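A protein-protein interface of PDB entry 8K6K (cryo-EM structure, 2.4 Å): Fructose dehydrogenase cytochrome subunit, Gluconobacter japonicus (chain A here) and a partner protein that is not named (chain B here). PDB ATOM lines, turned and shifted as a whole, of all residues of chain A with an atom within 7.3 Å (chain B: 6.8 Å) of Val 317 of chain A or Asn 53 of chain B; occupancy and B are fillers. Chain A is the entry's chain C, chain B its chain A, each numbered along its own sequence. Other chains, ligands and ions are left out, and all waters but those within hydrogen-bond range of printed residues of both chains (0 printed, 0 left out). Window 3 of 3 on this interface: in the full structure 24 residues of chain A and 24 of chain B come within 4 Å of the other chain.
OD1 of Asn 321 of chain A sits at hydrogen-bond distance from ND2 of Asn 53 of chain B (2.8 Å).
The guanidinium group (NH1) of Arg 324 of chain A is in hydrogen-bond range of the backbone carbonyl oxygen (O) of Asn 53 of chain B, 3.0 Å away.
NH2 of Arg 323 of chain A is in salt-bridge range of OE2 of Glu 49 of chain B (2.9 Å).
The side-chain amide oxygen (OD1) of Asn 50 of chain B sits close to the backbone carbonyl oxygen (O) of Arg 323 of chain A, 3.4 Å away.
The side-chain amide nitrogen (ND2) of Asn 53 of chain B is in hydrogen-bond range of the backbone carbonyl oxygen (O) of Val 317 of chain A (2.9 Å).
The guanidinium group of Arg 52 of chain B lies within hydrogen-bond range of the backbone carbonyl oxygen of Glu 340 of chain A (2.7 Å).
The backbone carbonyl oxygen of Arg 52 of chain B is in hydrogen-bond range of the side-chain amino group of Lys 59 of chain B, 3.0 Å away.
The backbone carbonyl oxygen of Asn 321 of chain A is in hydrogen-bond range of the guanidinium group of Arg 324 of chain A (3.3 Å).
The backbone carbonyl oxygen (O) of Ala 318 of chain A is in hydrogen-bond range of the side-chain amide nitrogen (ND2) of Asn 321 of chain A (2.9 Å).
CB of Ala 320 of chain A touches CD of Glu 49 of chain B, at 3.9 Å.
Ala 320 of chain A touches Asn 53 of chain B.
OD1 of Asn 50 of chain B touches CA of Arg 324 of chain A (3.6 Å).
Ser 316 of chain A touches none of the printed residues of chain B.
Val 317 of chain A touches one residue of chain B.
Asn 319 of chain A touches none of the printed residues of chain B.
Printed residues of chain B within 4 Å of Arg 324 of chain A: Asn 50 (3.6 Å) and Asn 53 (3.0 Å).
Printed residues of chain B within 4 Å of Glu 340 of chain A: Arg 52.
Printed residues of chain A within 4 Å of Glu 49 of chain B: Ala 320 (3.9 Å) and Arg 323 (2.9 Å).
Printed residues of chain A within 4 Å of Arg 52 of chain B: Glu 340.
Asn 53 of chain B touches just these residues of chain A: Val 317 (2.9 Å), Ala 320 (3.3 Å), Asn 321 (2.8 Å) and Arg 324 (3.0 Å).
The nearest residue of chain B that does not touch Val 317 of chain A is Arg 52 of chain B (5.2 Å).
The nearest printed residue of chain B that does not touch Arg 323 of chain A is Asn 53 of chain B (6.3 Å).
Of the 11 printed residues of chain A, 6 touch a printed residue of chain B.
Printed residues of chain A that touch a printed residue of chain B: Val 317, Ala 320, Asn 321, Arg 323, Arg 324 and Glu 340.
Of the 10 printed residues of chain B, 4 touch a printed residue of chain A.
Among the printed residues, 9 pairs touch across the chains.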
ATOM      1  N   TYR A 315      -5.188 -30.796 -26.827  1.00  0.00           N
ATOM      2  CA  TYR A 315      -5.249 -29.426 -27.309  1.00  0.00           C
ATOM      3  C   TYR A 315      -5.746 -28.513 -26.190  1.00  0.00           C
ATOM      4  O   TYR A 315      -5.858 -28.914 -25.030  1.00  0.00           O
ATOM      5  CB  TYR A 315      -6.136 -29.338 -28.551  1.00  0.00           C
ATOM      6  CG  TYR A 315      -7.624 -29.250 -28.288  1.00  0.00           C
ATOM      7  CD1 TYR A 315      -8.244 -30.069 -27.357  1.00  0.00           C
ATOM      8  CD2 TYR A 315      -8.407 -28.342 -28.985  1.00  0.00           C
ATOM      9  CE1 TYR A 315      -9.597 -29.976 -27.119  1.00  0.00           C
ATOM     10  CE2 TYR A 315      -9.759 -28.244 -28.756  1.00  0.00           C
ATOM     11  CZ  TYR A 315     -10.350 -29.063 -27.823  1.00  0.00           C
ATOM     12  OH  TYR A 315     -11.702 -28.969 -27.596  1.00  0.00           O
ATOM     13  N   SER A 316      -6.055 -27.267 -26.536  1.00  0.00           N
ATOM     14  CA  SER A 316      -6.621 -26.304 -25.606  1.00  0.00           C
ATOM     15  C   SER A 316      -7.927 -25.775 -26.176  1.00  0.00           C
ATOM     16  O   SER A 316      -7.955 -25.268 -27.302  1.00  0.00           O
ATOM     17  CB  SER A 316      -5.649 -25.151 -25.346  1.00  0.00           C
ATOM     18  OG  SER A 316      -6.076 -24.359 -24.254  1.00  0.00           O
ATOM     19  N   VAL A 317      -9.005 -25.903 -25.404  1.00  0.00           N
ATOM     20  CA  VAL A 317     -10.285 -25.341 -25.820  1.00  0.00           C
ATOM     21  C   VAL A 317     -10.217 -23.820 -25.831  1.00  0.00           C
ATOM     22  O   VAL A 317     -10.812 -23.164 -26.692  1.00  0.00           O
ATOM     23  CB  VAL A 317     -11.414 -25.851 -24.907  1.00  0.00           C
ATOM     24  CG1 VAL A 317     -12.765 -25.434 -25.449  1.00  0.00           C
ATOM     25  CG2 VAL A 317     -11.339 -27.358 -24.771  1.00  0.00           C
ATOM     26  N   ALA A 318      -9.488 -23.238 -24.876  1.00  0.00           N
ATOM     27  CA  ALA A 318      -9.412 -21.785 -24.775  1.00  0.00           C
ATOM     28  C   ALA A 318      -8.762 -21.171 -26.007  1.00  0.00           C
ATOM     29  O   ALA A 318      -9.165 -20.093 -26.458  1.00  0.00           O
ATOM     30  CB  ALA A 318      -8.647 -21.390 -23.513  1.00  0.00           C
ATOM     31  N   ASN A 319      -7.751 -21.839 -26.566  1.00  0.00           N
ATOM     32  CA  ASN A 319      -7.068 -21.311 -27.739  1.00  0.00           C
ATOM     33  C   ASN A 319      -7.957 -21.288 -28.973  1.00  0.00           C
ATOM     34  O   ASN A 319      -7.645 -20.574 -29.931  1.00  0.00           O
ATOM     35  CB  ASN A 319      -5.810 -22.130 -28.026  1.00  0.00           C
ATOM     36  CG  ASN A 319      -4.734 -21.928 -26.981  1.00  0.00           C
ATOM     37  OD1 ASN A 319      -4.869 -21.091 -26.091  1.00  0.00           O
ATOM     38  ND2 ASN A 319      -3.658 -22.696 -27.085  1.00  0.00           N
ATOM     39  N   ALA A 320      -9.050 -22.050 -28.978  1.00  0.00           N
ATOM     40  CA  ALA A 320      -9.938 -22.099 -30.130  1.00  0.00           C
ATOM     41  C   ALA A 320     -10.911 -20.932 -30.185  1.00  0.00           C
ATOM     42  O   ALA A 320     -11.576 -20.752 -31.209  1.00  0.00           O
ATOM     43  CB  ALA A 320     -10.719 -23.413 -30.134  1.00  0.00           C
ATOM     44  N   ASN A 321     -11.012 -20.142 -29.115  1.00  0.00           N
ATOM     45  CA  ASN A 321     -11.956 -19.029 -29.100  1.00  0.00           C
ATOM     46  C   ASN A 321     -11.590 -17.979 -30.140  1.00  0.00           C
ATOM     47  O   ASN A 321     -12.473 -17.377 -30.760  1.00  0.00           O
ATOM     48  CB  ASN A 321     -12.006 -18.409 -27.708  1.00  0.00           C
ATOM     49  CG  ASN A 321     -12.617 -19.335 -26.685  1.00  0.00           C
ATOM     50  OD1 ASN A 321     -13.719 -19.845 -26.874  1.00  0.00           O
ATOM     51  ND2 ASN A 321     -11.903 -19.562 -25.591  1.00  0.00           N
ATOM     52  N   SER A 322     -10.293 -17.738 -30.336  1.00  0.00           N
ATOM     53  CA  SER A 322      -9.857 -16.794 -31.353  1.00  0.00           C
ATOM     54  C   SER A 322     -10.209 -17.255 -32.760  1.00  0.00           C
ATOM     55  O   SER A 322     -10.303 -16.422 -33.666  1.00  0.00           O
ATOM     56  CB  SER A 322      -8.350 -16.570 -31.245  1.00  0.00           C
ATOM     57  OG  SER A 322      -7.641 -17.752 -31.565  1.00  0.00           O
ATOM     58  N   ARG A 323     -10.410 -18.554 -32.959  1.00  0.00           N
ATOM     59  CA  ARG A 323     -10.721 -19.102 -34.270  1.00  0.00           C
ATOM     60  C   ARG A 323     -12.217 -19.196 -34.527  1.00  0.00           C
ATOM     61  O   ARG A 323     -12.623 -19.770 -35.541  1.00  0.00           O
ATOM     62  CB  ARG A 323     -10.073 -20.476 -34.436  1.00  0.00           C
ATOM     63  CG  ARG A 323      -8.624 -20.409 -34.875  1.00  0.00           C
ATOM     64  CD  ARG A 323      -8.063 -21.785 -35.160  1.00  0.00           C
ATOM     65  NE  ARG A 323      -8.488 -22.769 -34.172  1.00  0.00           N
ATOM     66  CZ  ARG A 323      -7.791 -23.091 -33.093  1.00  0.00           C
ATOM     67  NH1 ARG A 323      -6.638 -22.508 -32.815  1.00  0.00           N
ATOM     68  NH2 ARG A 323      -8.261 -24.027 -32.273  1.00  0.00           N
ATOM     69  N   ARG A 324     -13.044 -18.678 -33.627  1.00  0.00           N
ATOM     70  CA  ARG A 324     -14.450 -18.515 -33.948  1.00  0.00           C
ATOM     71  C   ARG A 324     -14.610 -17.391 -34.964  1.00  0.00           C
ATOM     72  O   ARG A 324     -13.744 -16.523 -35.109  1.00  0.00           O
ATOM     73  CB  ARG A 324     -15.264 -18.231 -32.687  1.00  0.00           C
ATOM     74  CG  ARG A 324     -15.224 -19.359 -31.672  1.00  0.00           C
ATOM     75  CD  ARG A 324     -16.058 -19.046 -30.448  1.00  0.00           C
ATOM     76  NE  ARG A 324     -15.567 -17.878 -29.731  1.00  0.00           N
ATOM     77  CZ  ARG A 324     -15.994 -17.500 -28.534  1.00  0.00           C
ATOM     78  NH1 ARG A 324     -16.918 -18.184 -27.883  1.00  0.00           N
ATOM     79  NH2 ARG A 324     -15.479 -16.407 -27.978  1.00  0.00           N
ATOM     80  N   GLU A 340      -8.509 -32.426 -33.203  1.00  0.00           N
ATOM     81  CA  GLU A 340      -9.744 -32.328 -32.440  1.00  0.00           C
ATOM     82  C   GLU A 340     -10.926 -31.985 -33.335  1.00  0.00           C
ATOM     83  O   GLU A 340     -12.010 -32.561 -33.194  1.00  0.00           O
ATOM     84  CB  GLU A 340      -9.601 -31.294 -31.328  1.00  0.00           C
ATOM     85  CG  GLU A 340     -10.760 -31.301 -30.357  1.00  0.00           C
ATOM     86  CD  GLU A 340     -10.597 -32.337 -29.271  1.00  0.00           C
ATOM     87  OE1 GLU A 340      -9.519 -32.959 -29.198  1.00  0.00           O
ATOM     88  OE2 GLU A 340     -11.547 -32.530 -28.486  1.00  0.00           O
ATOM     89  N   VAL B  48     -17.732 -27.368 -36.611  1.00  0.00           N
ATOM     90  CA  VAL B  48     -17.773 -28.195 -35.408  1.00  0.00           C
ATOM     91  C   VAL B  48     -17.004 -27.525 -34.279  1.00  0.00           C
ATOM     92  O   VAL B  48     -17.467 -27.467 -33.134  1.00  0.00           O
ATOM     93  CB  VAL B  48     -17.219 -29.598 -35.707  1.00  0.00           C
ATOM     94  CG1 VAL B  48     -17.103 -30.404 -34.432  1.00  0.00           C
ATOM     95  CG2 VAL B  48     -18.103 -30.303 -36.698  1.00  0.00           C
ATOM     96  N   GLU B  49     -15.814 -27.013 -34.588  1.00  0.00           N
ATOM     97  CA  GLU B  49     -15.020 -26.321 -33.578  1.00  0.00           C
ATOM     98  C   GLU B  49     -15.728 -25.066 -33.087  1.00  0.00           C
ATOM     99  O   GLU B  49     -15.683 -24.744 -31.895  1.00  0.00           O
ATOM    100  CB  GLU B  49     -13.643 -25.974 -34.139  1.00  0.00           C
ATOM    101  CG  GLU B  49     -12.670 -25.464 -33.097  1.00  0.00           C
ATOM    102  CD  GLU B  49     -11.508 -24.717 -33.709  1.00  0.00           C
ATOM    103  OE1 GLU B  49     -11.712 -23.578 -34.172  1.00  0.00           O
ATOM    104  OE2 GLU B  49     -10.390 -25.270 -33.727  1.00  0.00           O
ATOM    105  N   ASN B  50     -16.377 -24.337 -33.997  1.00  0.00           N
ATOM    106  CA  ASN B  50     -17.123 -23.147 -33.604  1.00  0.00           C
ATOM    107  C   ASN B  50     -18.273 -23.501 -32.674  1.00  0.00           C
ATOM    108  O   ASN B  50     -18.535 -22.786 -31.701  1.00  0.00           O
ATOM    109  CB  ASN B  50     -17.644 -22.424 -34.845  1.00  0.00           C
ATOM    110  CG  ASN B  50     -16.542 -21.757 -35.633  1.00  0.00           C
ATOM    111  OD1 ASN B  50     -15.385 -21.753 -35.221  1.00  0.00           O
ATOM    112  ND2 ASN B  50     -16.895 -21.190 -36.778  1.00  0.00           N
ATOM    113  N   TRP B  51     -18.981 -24.593 -32.964  1.00  0.00           N
ATOM    114  CA  TRP B  51     -20.070 -25.013 -32.089  1.00  0.00           C
ATOM    115  C   TRP B  51     -19.549 -25.455 -30.730  1.00  0.00           C
ATOM    116  O   TRP B  51     -20.152 -25.141 -29.699  1.00  0.00           O
ATOM    117  CB  TRP B  51     -20.879 -26.136 -32.733  1.00  0.00           C
ATOM    118  CG  TRP B  51     -22.051 -26.535 -31.895  1.00  0.00           C
ATOM    119  CD1 TRP B  51     -23.298 -25.996 -31.930  1.00  0.00           C
ATOM    120  CD2 TRP B  51     -22.079 -27.542 -30.878  1.00  0.00           C
ATOM    121  NE1 TRP B  51     -24.105 -26.607 -31.007  1.00  0.00           N
ATOM    122  CE2 TRP B  51     -23.379 -27.562 -30.347  1.00  0.00           C
ATOM    123  CE3 TRP B  51     -21.131 -28.431 -30.368  1.00  0.00           C
ATOM    124  CZ2 TRP B  51     -23.757 -28.434 -29.333  1.00  0.00           C
ATOM    125  CZ3 TRP B  51     -21.506 -29.295 -29.365  1.00  0.00           C
ATOM    126  CH2 TRP B  51     -22.807 -29.291 -28.857  1.00  0.00           C
ATOM    127  N   ARG B  52     -18.438 -26.192 -30.708  1.00  0.00           N
ATOM    128  CA  ARG B  52     -17.889 -26.662 -29.442  1.00  0.00           C
ATOM    129  C   ARG B  52     -17.478 -25.503 -28.548  1.00  0.00           C
ATOM    130  O   ARG B  52     -17.587 -25.596 -27.320  1.00  0.00           O
ATOM    131  CB  ARG B  52     -16.697 -27.580 -29.695  1.00  0.00           C
ATOM    132  CG  ARG B  52     -17.074 -28.969 -30.155  1.00  0.00           C
ATOM    133  CD  ARG B  52     -15.913 -29.636 -30.859  1.00  0.00           C
ATOM    134  NE  ARG B  52     -16.179 -31.041 -31.136  1.00  0.00           N
ATOM    135  CZ  ARG B  52     -15.365 -31.835 -31.816  1.00  0.00           C
ATOM    136  NH1 ARG B  52     -14.217 -31.396 -32.298  1.00  0.00           N
ATOM    137  NH2 ARG B  52     -15.717 -33.100 -32.023  1.00  0.00           N
ATOM    138  N   ASN B  53     -17.006 -24.411 -29.139  1.00  0.00           N
ATOM    139  CA  ASN B  53     -16.613 -23.226 -28.394  1.00  0.00           C
ATOM    140  C   ASN B  53     -17.738 -22.210 -28.272  1.00  0.00           C
ATOM    141  O   ASN B  53     -17.509 -21.107 -27.771  1.00  0.00           O
ATOM    142  CB  ASN B  53     -15.390 -22.583 -29.044  1.00  0.00           C
ATOM    143  CG  ASN B  53     -14.095 -23.191 -28.561  1.00  0.00           C
ATOM    144  OD1 ASN B  53     -13.690 -24.256 -29.020  1.00  0.00           O
ATOM    145  ND2 ASN B  53     -13.441 -22.522 -27.622  1.00  0.00           N
ATOM    146  N   MET B  54     -18.934 -22.547 -28.738  1.00  0.00           N
ATOM    147  CA  MET B  54     -20.088 -21.704 -28.486  1.00  0.00           C
ATOM    148  C   MET B  54     -20.506 -21.848 -27.023  1.00  0.00           C
ATOM    149  O   MET B  54     -20.436 -22.948 -26.468  1.00  0.00           O
ATOM    150  CB  MET B  54     -21.238 -22.097 -29.414  1.00  0.00           C
ATOM    151  CG  MET B  54     -22.337 -21.065 -29.537  1.00  0.00           C
ATOM    152  SD  MET B  54     -23.676 -21.575 -30.625  1.00  0.00           S
ATOM    153  CE  MET B  54     -23.935 -23.250 -30.070  1.00  0.00           C
ATOM    154  N   PRO B  55     -20.921 -20.764 -26.371  1.00  0.00           N
ATOM    155  CA  PRO B  55     -21.217 -20.844 -24.944  1.00  0.00           C
ATOM    156  C   PRO B  55     -22.321 -21.841 -24.668  1.00  0.00           C
ATOM    157  O   PRO B  55     -23.231 -22.037 -25.497  1.00  0.00           O
ATOM    158  CB  PRO B  55     -21.646 -19.413 -24.595  1.00  0.00           C
ATOM    159  CG  PRO B  55     -20.915 -18.582 -25.563  1.00  0.00           C
ATOM    160  CD  PRO B  55     -20.892 -19.371 -26.840  1.00  0.00           C
ATOM    161  N   PRO B  56     -22.278 -22.510 -23.513  1.00  0.00           N
ATOM    162  CA  PRO B  56     -23.285 -23.542 -23.221  1.00  0.00           C
ATOM    163  C   PRO B  56     -24.706 -23.016 -23.176  1.00  0.00           C
ATOM    164  O   PRO B  56     -25.644 -23.789 -23.394  1.00  0.00           O
ATOM    165  CB  PRO B  56     -22.842 -24.080 -21.854  1.00  0.00           C
ATOM    166  CG  PRO B  56     -22.014 -22.997 -21.267  1.00  0.00           C
ATOM    167  CD  PRO B  56     -21.312 -22.357 -22.416  1.00  0.00           C
ATOM    168  N   LYS B  59     -26.043 -23.455 -26.429  1.00  0.00           N
ATOM    169  CA  LYS B  59     -26.354 -24.843 -26.736  1.00  0.00           C
ATOM    170  C   LYS B  59     -27.655 -25.280 -26.082  1.00  0.00           C
ATOM    171  O   LYS B  59     -28.412 -26.061 -26.666  1.00  0.00           O
ATOM    172  CB  LYS B  59     -25.217 -25.758 -26.278  1.00  0.00           C
ATOM    173  CG  LYS B  59     -23.890 -25.526 -26.967  1.00  0.00           C
ATOM    174  CD  LYS B  59     -22.807 -26.366 -26.314  1.00  0.00           C
ATOM    175  CE  LYS B  59     -21.494 -26.269 -27.058  1.00  0.00           C
ATOM    176  NZ  LYS B  59     -20.412 -25.723 -26.201  1.00  0.00           N
